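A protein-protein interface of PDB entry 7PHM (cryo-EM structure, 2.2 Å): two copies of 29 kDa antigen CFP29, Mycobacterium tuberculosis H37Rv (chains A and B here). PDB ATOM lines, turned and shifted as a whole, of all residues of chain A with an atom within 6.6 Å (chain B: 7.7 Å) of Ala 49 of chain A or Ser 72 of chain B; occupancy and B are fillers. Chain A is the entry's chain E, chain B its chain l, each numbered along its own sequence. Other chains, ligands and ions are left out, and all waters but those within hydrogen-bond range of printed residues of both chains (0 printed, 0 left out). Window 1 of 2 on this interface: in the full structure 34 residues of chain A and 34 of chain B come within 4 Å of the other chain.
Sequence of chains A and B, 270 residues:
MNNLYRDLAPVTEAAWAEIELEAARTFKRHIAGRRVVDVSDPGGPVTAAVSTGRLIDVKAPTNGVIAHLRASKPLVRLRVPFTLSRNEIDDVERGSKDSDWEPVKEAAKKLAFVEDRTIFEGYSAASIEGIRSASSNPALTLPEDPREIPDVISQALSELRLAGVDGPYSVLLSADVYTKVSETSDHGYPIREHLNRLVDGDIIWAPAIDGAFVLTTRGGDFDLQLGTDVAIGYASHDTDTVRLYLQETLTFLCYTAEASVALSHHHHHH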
ATOM      1  N   VAL A  46       5.435  -5.093  26.950  1.00  0.00           N
ATOM      2  CA  VAL A  46       6.663  -5.787  26.600  1.00  0.00           C
ATOM      3  C   VAL A  46       6.372  -7.183  26.064  1.00  0.00           C
ATOM      4  O   VAL A  46       7.021  -7.610  25.107  1.00  0.00           O
ATOM      5  CB  VAL A  46       7.629  -5.807  27.799  1.00  0.00           C
ATOM      6  CG1 VAL A  46       8.894  -6.591  27.489  1.00  0.00           C
ATOM      7  CG2 VAL A  46       8.006  -4.395  28.177  1.00  0.00           C
ATOM      8  N   THR A  47       5.357  -7.872  26.599  1.00  0.00           N
ATOM      9  CA  THR A  47       5.172  -9.298  26.335  1.00  0.00           C
ATOM     10  C   THR A  47       4.837  -9.563  24.869  1.00  0.00           C
ATOM     11  O   THR A  47       4.020  -8.874  24.255  1.00  0.00           O
ATOM     12  CB  THR A  47       4.119  -9.905  27.273  1.00  0.00           C
ATOM     13  OG1 THR A  47       3.948 -11.299  26.981  1.00  0.00           O
ATOM     14  CG2 THR A  47       2.803  -9.232  27.197  1.00  0.00           C
ATOM     15  N   ALA A  48       5.555 -10.508  24.294  1.00  0.00           N
ATOM     16  CA  ALA A  48       5.528 -10.750  22.871  1.00  0.00           C
ATOM     17  C   ALA A  48       5.153 -12.171  22.513  1.00  0.00           C
ATOM     18  O   ALA A  48       4.782 -12.420  21.365  1.00  0.00           O
ATOM     19  CB  ALA A  48       6.896 -10.434  22.254  1.00  0.00           C
ATOM     20  N   ALA A  49       5.258 -13.106  23.446  1.00  0.00           N
ATOM     21  CA  ALA A  49       4.998 -14.501  23.156  1.00  0.00           C
ATOM     22  C   ALA A  49       4.453 -15.166  24.405  1.00  0.00           C
ATOM     23  O   ALA A  49       4.653 -14.694  25.522  1.00  0.00           O
ATOM     24  CB  ALA A  49       6.254 -15.221  22.656  1.00  0.00           C
ATOM     25  N   VAL A  50       3.742 -16.263  24.196  1.00  0.00           N
ATOM     26  CA  VAL A  50       3.225 -17.098  25.269  1.00  0.00           C
ATOM     27  C   VAL A  50       3.898 -18.451  25.151  1.00  0.00           C
ATOM     28  O   VAL A  50       3.810 -19.098  24.105  1.00  0.00           O
ATOM     29  CB  VAL A  50       1.698 -17.244  25.203  1.00  0.00           C
ATOM     30  CG1 VAL A  50       1.224 -18.254  26.220  1.00  0.00           C
ATOM     31  CG2 VAL A  50       1.040 -15.919  25.441  1.00  0.00           C
ATOM     32  N   SER A  51       4.554 -18.875  26.221  1.00  0.00           N
ATOM     33  CA  SER A  51       5.180 -20.187  26.267  1.00  0.00           C
ATOM     34  C   SER A  51       4.144 -21.298  26.187  1.00  0.00           C
ATOM     35  O   SER A  51       3.147 -21.283  26.905  1.00  0.00           O
ATOM     36  CB  SER A  51       5.966 -20.328  27.556  1.00  0.00           C
ATOM     37  OG  SER A  51       6.548 -21.611  27.648  1.00  0.00           O
ATOM     38  N   SER A  72       6.787 -21.408  21.491  1.00  0.00           N
ATOM     39  CA  SER A  72       5.939 -20.346  22.001  1.00  0.00           C
ATOM     40  C   SER A  72       4.978 -19.900  20.912  1.00  0.00           C
ATOM     41  O   SER A  72       5.132 -20.235  19.740  1.00  0.00           O
ATOM     42  CB  SER A  72       6.760 -19.159  22.521  1.00  0.00           C
ATOM     43  OG  SER A  72       7.518 -18.570  21.489  1.00  0.00           O
ATOM     44  N   LYS A  73       3.970 -19.145  21.325  1.00  0.00           N
ATOM     45  CA  LYS A  73       2.981 -18.587  20.421  1.00  0.00           C
ATOM     46  C   LYS A  73       3.112 -17.077  20.396  1.00  0.00           C
ATOM     47  O   LYS A  73       3.051 -16.451  21.456  1.00  0.00           O
ATOM     48  CB  LYS A  73       1.574 -18.990  20.845  1.00  0.00           C
ATOM     49  CG  LYS A  73       1.258 -20.444  20.628  1.00  0.00           C
ATOM     50  CD  LYS A  73       1.167 -20.733  19.149  1.00  0.00           C
ATOM     51  CE  LYS A  73       0.732 -22.149  18.882  1.00  0.00           C
ATOM     52  NZ  LYS A  73       0.678 -22.437  17.429  1.00  0.00           N
ATOM     53  N   PRO A  74       3.277 -16.455  19.238  1.00  0.00           N
ATOM     54  CA  PRO A  74       3.423 -14.999  19.200  1.00  0.00           C
ATOM     55  C   PRO A  74       2.099 -14.298  19.437  1.00  0.00           C
ATOM     56  O   PRO A  74       1.028 -14.799  19.103  1.00  0.00           O
ATOM     57  CB  PRO A  74       3.937 -14.738  17.784  1.00  0.00           C
ATOM     58  CG  PRO A  74       3.376 -15.858  16.997  1.00  0.00           C
ATOM     59  CD  PRO A  74       3.363 -17.050  17.897  1.00  0.00           C
ATOM     60  N   LEU A  75       2.184 -13.133  20.045  1.00  0.00           N
ATOM     61  CA  LEU A  75       1.033 -12.259  20.156  1.00  0.00           C
ATOM     62  C   LEU A  75       0.912 -11.437  18.887  1.00  0.00           C
ATOM     63  O   LEU A  75       1.897 -11.154  18.211  1.00  0.00           O
ATOM     64  CB  LEU A  75       1.151 -11.354  21.374  1.00  0.00           C
ATOM     65  CG  LEU A  75       0.705 -11.899  22.732  1.00  0.00           C
ATOM     66  CD1 LEU A  75       1.626 -12.945  23.297  1.00  0.00           C
ATOM     67  CD2 LEU A  75       0.647 -10.773  23.675  1.00  0.00           C
ATOM     68  N   THR A 251      -3.169 -13.167  21.835  1.00  0.00           N
ATOM     69  CA  THR A 251      -3.220 -14.420  21.103  1.00  0.00           C
ATOM     70  C   THR A 251      -4.249 -15.293  21.801  1.00  0.00           C
ATOM     71  O   THR A 251      -4.664 -15.010  22.923  1.00  0.00           O
ATOM     72  CB  THR A 251      -1.849 -15.109  21.028  1.00  0.00           C
ATOM     73  OG1 THR A 251      -1.923 -16.227  20.143  1.00  0.00           O
ATOM     74  CG2 THR A 251      -1.395 -15.581  22.383  1.00  0.00           C
ATOM     75  N   ALA B  48      10.057 -18.982  27.564  1.00  0.00           N
ATOM     76  CA  ALA B  48      10.359 -19.625  26.308  1.00  0.00           C
ATOM     77  C   ALA B  48      10.878 -18.670  25.256  1.00  0.00           C
ATOM     78  O   ALA B  48      11.469 -19.124  24.276  1.00  0.00           O
ATOM     79  CB  ALA B  48       9.112 -20.327  25.757  1.00  0.00           C
ATOM     80  N   ALA B  49      10.662 -17.372  25.419  1.00  0.00           N
ATOM     81  CA  ALA B  49      11.054 -16.404  24.416  1.00  0.00           C
ATOM     82  C   ALA B  49      11.400 -15.098  25.105  1.00  0.00           C
ATOM     83  O   ALA B  49      10.969 -14.832  26.225  1.00  0.00           O
ATOM     84  CB  ALA B  49       9.958 -16.196  23.367  1.00  0.00           C
ATOM     85  N   VAL B  50      12.203 -14.295  24.424  1.00  0.00           N
ATOM     86  CA  VAL B  50      12.563 -12.960  24.870  1.00  0.00           C
ATOM     87  C   VAL B  50      12.007 -11.981  23.855  1.00  0.00           C
ATOM     88  O   VAL B  50      12.325 -12.072  22.668  1.00  0.00           O
ATOM     89  CB  VAL B  50      14.082 -12.789  25.013  1.00  0.00           C
ATOM     90  CG1 VAL B  50      14.421 -11.347  25.303  1.00  0.00           C
ATOM     91  CG2 VAL B  50      14.605 -13.675  26.102  1.00  0.00           C
ATOM     92  N   SER B  51      11.192 -11.048  24.327  1.00  0.00           N
ATOM     93  CA  SER B  51      10.650 -10.002  23.473  1.00  0.00           C
ATOM     94  C   SER B  51      11.748  -9.092  22.945  1.00  0.00           C
ATOM     95  O   SER B  51      12.593  -8.620  23.701  1.00  0.00           O
ATOM     96  CB  SER B  51       9.650  -9.177  24.259  1.00  0.00           C
ATOM     97  OG  SER B  51       9.140  -8.124  23.467  1.00  0.00           O
ATOM     98  N   THR B  52      11.731  -8.846  21.646  1.00  0.00           N
ATOM     99  CA  THR B  52      12.624  -7.862  21.062  1.00  0.00           C
ATOM    100  C   THR B  52      11.992  -6.485  20.964  1.00  0.00           C
ATOM    101  O   THR B  52      12.663  -5.543  20.545  1.00  0.00           O
ATOM    102  CB  THR B  52      13.075  -8.297  19.671  1.00  0.00           C
ATOM    103  OG1 THR B  52      11.961  -8.290  18.781  1.00  0.00           O
ATOM    104  CG2 THR B  52      13.649  -9.689  19.721  1.00  0.00           C
ATOM    105  N   GLY B  53      10.715  -6.354  21.310  1.00  0.00           N
ATOM    106  CA  GLY B  53       9.994  -5.113  21.178  1.00  0.00           C
ATOM    107  C   GLY B  53       9.610  -4.723  19.771  1.00  0.00           C
ATOM    108  O   GLY B  53       8.961  -3.696  19.595  1.00  0.00           O
ATOM    109  N   ARG B  54       9.973  -5.500  18.763  1.00  0.00           N
ATOM    110  CA  ARG B  54       9.704  -5.096  17.397  1.00  0.00           C
ATOM    111  C   ARG B  54       8.436  -5.746  16.857  1.00  0.00           C
ATOM    112  O   ARG B  54       7.828  -6.612  17.482  1.00  0.00           O
ATOM    113  CB  ARG B  54      10.903  -5.406  16.512  1.00  0.00           C
ATOM    114  CG  ARG B  54      12.054  -4.497  16.849  1.00  0.00           C
ATOM    115  CD  ARG B  54      13.266  -4.714  16.003  1.00  0.00           C
ATOM    116  NE  ARG B  54      14.335  -3.842  16.467  1.00  0.00           N
ATOM    117  CZ  ARG B  54      14.538  -2.609  16.020  1.00  0.00           C
ATOM    118  NH1 ARG B  54      13.757  -2.105  15.079  1.00  0.00           N
ATOM    119  NH2 ARG B  54      15.528  -1.885  16.507  1.00  0.00           N
ATOM    120  N   LEU B  55       8.030  -5.285  15.683  1.00  0.00           N
ATOM    121  CA  LEU B  55       6.799  -5.699  15.039  1.00  0.00           C
ATOM    122  C   LEU B  55       7.132  -6.332  13.701  1.00  0.00           C
ATOM    123  O   LEU B  55       8.088  -5.935  13.040  1.00  0.00           O
ATOM    124  CB  LEU B  55       5.865  -4.513  14.831  1.00  0.00           C
ATOM    125  CG  LEU B  55       5.445  -3.736  16.074  1.00  0.00           C
ATOM    126  CD1 LEU B  55       4.595  -2.541  15.698  1.00  0.00           C
ATOM    127  CD2 LEU B  55       4.721  -4.615  17.035  1.00  0.00           C
ATOM    128  N   ILE B  56       6.347  -7.320  13.308  1.00  0.00           N
ATOM    129  CA  ILE B  56       6.502  -7.977  12.022  1.00  0.00           C
ATOM    130  C   ILE B  56       5.211  -7.778  11.255  1.00  0.00           C
ATOM    131  O   ILE B  56       4.132  -8.051  11.786  1.00  0.00           O
ATOM    132  CB  ILE B  56       6.825  -9.472  12.178  1.00  0.00           C
ATOM    133  CG1 ILE B  56       8.103  -9.652  12.995  1.00  0.00           C
ATOM    134  CG2 ILE B  56       6.967 -10.129  10.820  1.00  0.00           C
ATOM    135  CD1 ILE B  56       8.324 -11.052  13.460  1.00  0.00           C
ATOM    136  N   LEU B  69       2.616  -8.980  14.051  1.00  0.00           N
ATOM    137  CA  LEU B  69       3.111  -9.958  15.000  1.00  0.00           C
ATOM    138  C   LEU B  69       4.181  -9.338  15.875  1.00  0.00           C
ATOM    139  O   LEU B  69       5.033  -8.584  15.409  1.00  0.00           O
ATOM    140  CB  LEU B  69       3.680 -11.180  14.290  1.00  0.00           C
ATOM    141  CG  LEU B  69       2.660 -12.061  13.595  1.00  0.00           C
ATOM    142  CD1 LEU B  69       3.359 -13.158  12.832  1.00  0.00           C
ATOM    143  CD2 LEU B  69       1.717 -12.628  14.630  1.00  0.00           C
ATOM    144  N   ARG B  70       4.125  -9.655  17.155  1.00  0.00           N
ATOM    145  CA  ARG B  70       5.182  -9.289  18.076  1.00  0.00           C
ATOM    146  C   ARG B  70       6.385 -10.192  17.827  1.00  0.00           C
ATOM    147  O   ARG B  70       6.249 -11.415  17.790  1.00  0.00           O
ATOM    148  CB  ARG B  70       4.702  -9.392  19.516  1.00  0.00           C
ATOM    149  CG  ARG B  70       3.657  -8.378  19.896  1.00  0.00           C
ATOM    150  CD  ARG B  70       4.226  -6.979  19.800  1.00  0.00           C
ATOM    151  NE  ARG B  70       5.394  -6.807  20.647  1.00  0.00           N
ATOM    152  CZ  ARG B  70       5.368  -6.321  21.878  1.00  0.00           C
ATOM    153  NH1 ARG B  70       6.486  -6.225  22.565  1.00  0.00           N
ATOM    154  NH2 ARG B  70       4.242  -5.895  22.406  1.00  0.00           N
ATOM    155  N   ALA B  71       7.546  -9.588  17.618  1.00  0.00           N
ATOM    156  CA  ALA B  71       8.768 -10.342  17.391  1.00  0.00           C
ATOM    157  C   ALA B  71       9.394 -10.767  18.711  1.00  0.00           C
ATOM    158  O   ALA B  71       9.305 -10.060  19.715  1.00  0.00           O
ATOM    159  CB  ALA B  71       9.766  -9.516  16.586  1.00  0.00           C
ATOM    160  N   SER B  72      10.023 -11.935  18.703  1.00  0.00           N
ATOM    161  CA  SER B  72      10.697 -12.438  19.886  1.00  0.00           C
ATOM    162  C   SER B  72      11.813 -13.382  19.470  1.00  0.00           C
ATOM    163  O   SER B  72      11.897 -13.812  18.322  1.00  0.00           O
ATOM    164  CB  SER B  72       9.723 -13.135  20.845  1.00  0.00           C
ATOM    165  OG  SER B  72       9.133 -14.265  20.241  1.00  0.00           O
ATOM    166  N   LYS B  73      12.680 -13.684  20.425  1.00  0.00           N
ATOM    167  CA  LYS B  73      13.783 -14.607  20.225  1.00  0.00           C
ATOM    168  C   LYS B  73      13.567 -15.846  21.072  1.00  0.00           C
ATOM    169  O   LYS B  73      13.394 -15.720  22.285  1.00  0.00           O
ATOM    170  CB  LYS B  73      15.110 -13.947  20.579  1.00  0.00           C
ATOM    171  CG  LYS B  73      15.548 -12.885  19.607  1.00  0.00           C
ATOM    172  CD  LYS B  73      15.926 -13.518  18.291  1.00  0.00           C
ATOM    173  CE  LYS B  73      16.488 -12.511  17.325  1.00  0.00           C
ATOM    174  NZ  LYS B  73      16.824 -13.133  16.023  1.00  0.00           N
ATOM    175  N   PRO B  74      13.580 -17.039  20.498  1.00  0.00           N
ATOM    176  CA  PRO B  74      13.355 -18.243  21.300  1.00  0.00           C
ATOM    177  C   PRO B  74      14.569 -18.587  22.144  1.00  0.00           C
ATOM    178  O   PRO B  74      15.712 -18.315  21.782  1.00  0.00           O
ATOM    179  CB  PRO B  74      13.096 -19.320  20.247  1.00  0.00           C
ATOM    180  CG  PRO B  74      13.859 -18.848  19.070  1.00  0.00           C
ATOM    181  CD  PRO B  74      13.779 -17.356  19.077  1.00  0.00           C
ATOM    182  N   LEU B  75      14.304 -19.171  23.294  1.00  0.00           N
ATOM    183  CA  LEU B  75      15.359 -19.740  24.107  1.00  0.00           C
ATOM    184  C   LEU B  75      15.660 -21.143  23.616  1.00  0.00           C
ATOM    185  O   LEU B  75      14.801 -21.829  23.071  1.00  0.00           O
ATOM    186  CB  LEU B  75      14.965 -19.756  25.577  1.00  0.00           C
ATOM    187  CG  LEU B  75      15.186 -18.489  26.406  1.00  0.00           C
ATOM    188  CD1 LEU B  75      14.242 -17.370  26.063  1.00  0.00           C
ATOM    189  CD2 LEU B  75      15.002 -18.836  27.822  1.00  0.00           C
ATOM    190  N   SER B 127      18.384 -19.064  16.052  1.00  0.00           N
ATOM    191  CA  SER B 127      18.207 -17.654  15.679  1.00  0.00           C
ATOM    192  C   SER B 127      19.097 -16.735  16.510  1.00  0.00           C
ATOM    193  O   SER B 127      18.713 -15.626  16.867  1.00  0.00           O
ATOM    194  CB  SER B 127      16.740 -17.222  15.773  1.00  0.00           C
ATOM    195  OG  SER B 127      15.953 -17.918  14.835  1.00  0.00           O
ATOM    196  N   LEU B 253      21.533 -12.087  23.054  1.00  0.00           N
ATOM    197  CA  LEU B 253      21.158 -10.942  22.237  1.00  0.00           C
ATOM    198  C   LEU B 253      22.279  -9.921  22.295  1.00  0.00           C
ATOM    199  O   LEU B 253      22.760  -9.585  23.379  1.00  0.00           O
ATOM    200  CB  LEU B 253      19.845 -10.306  22.707  1.00  0.00           C
ATOM    201  CG  LEU B 253      18.522 -11.046  22.494  1.00  0.00           C
ATOM    202  CD1 LEU B 253      18.267 -12.033  23.606  1.00  0.00           C
ATOM    203  CD2 LEU B 253      17.353 -10.105  22.347  1.00  0.00           C
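The backbone carbonyl oxygen (O) of Val 46 of chain A sits at hydrogen-bond distance from the side-chain hydroxyl (OG) of Ser 51 of chain B (2.7 Å).
O of Val 46 of chain A is in hydrogen-bond range of NH1 of Arg 70 of chain B, at 2.9 Å.
The backbone carbonyl oxygen of Leu 75 of chain A is in hydrogen-bond range of the backbone NH of Arg 70 of chain B, 2.9 Å away.
N of Leu 75 of chain A sits at hydrogen-bond distance from O of Ala 48 of chain A, at 3.0 Å.
The backbone carbonyl oxygen (O) of Ala 48 of chain B lies within hydrogen-bond range of the backbone NH (N) of Leu 75 of chain B (3.0 Å).
The side-chain hydroxyl (OG) of Ser 51 of chain B is in hydrogen-bond range of the backbone NH (N) of Gly 53 of chain B.
The side-chain hydroxyl of Ser 51 of chain B is in hydrogen-bond range of the guanidinium group of Arg 70 of chain B (3.4 Å).
The side-chain hydroxyl (OG1) of Thr 52 of chain B sits at hydrogen-bond distance from the backbone carbonyl oxygen (O) of Ala 71 of chain B, at 3.3 Å.
The backbone NH of Ile 56 of chain B is in hydrogen-bond range of the backbone carbonyl oxygen of Leu 69 of chain B (2.8 Å).
Among the printed residues, pairs that only touch across the chains: Ser 51 of chain A with Ala 48 of chain B, Ala 48 of chain A with Ser 51 of chain B, Thr 47 of chain A with Arg 70 of chain B, Ala 48 of chain A with Ala 71 of chain B, Ala 48 of chain A with Arg 70 of chain B, Leu 75 of chain A with Leu 69 of chain B, Ala 49 of chain A with Ser 72 of chain B, Ser 72 of chain A with Ala 49 of chain B and Ala 49 of chain A with Ala 49 of chain B.
Ala 49 of chain A touches just these residues of chain B: Ala 49 and Ser 72.
Printed residues of chain A within 4 Å of Ser 72 of chain B: Ala 49.
Of the printed residues of chain A, Ala 48 of chain B touches Ser 51.
Of the printed residues of chain A, Ala 49 of chain B touches Ala 49 (3.9 Å) and Ser 72 (3.9 Å).
Pro 74 of chain A touches none of the printed residues of chain B.
The nearest printed residue of chain B that does not touch Leu 75 of chain A is Ala 71 of chain B (5.9 Å).
Of the 18 printed residues of chain B, 7 touch a printed residue of chain A.
Of the 11 printed residues of chain A, 7 touch a printed residue of chain B.
Printed residues of chain A that touch a printed residue of chain B: Val 46, Thr 47, Ala 48, Ala 49, Ser 51, Ser 72 and Leu 75.
Hydrophobic or aromatic side chains of chain A that line the printed part of chain B: Ala 48 and Ala 49.
Among the printed residues, 12 pairs touch across the chains.
Among the printed residues, no Asp or Glu carboxylate lies within 4 Å of a Lys or Arg side-chain nitrogen of the other chain.
Ala 48 of chain A touches Ser 51 of chain B, and with the chains exchanged Ser 51 of chain A touches Ala 48 of chain B.
Ala 49 of chain A touches its own counterpart, Ala 49 of chain B.
Ala 49 of chain A touches Ser 72 of chain B, and with the chains exchanged Ser 72 of chain A touches Ala 49 of chain B.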
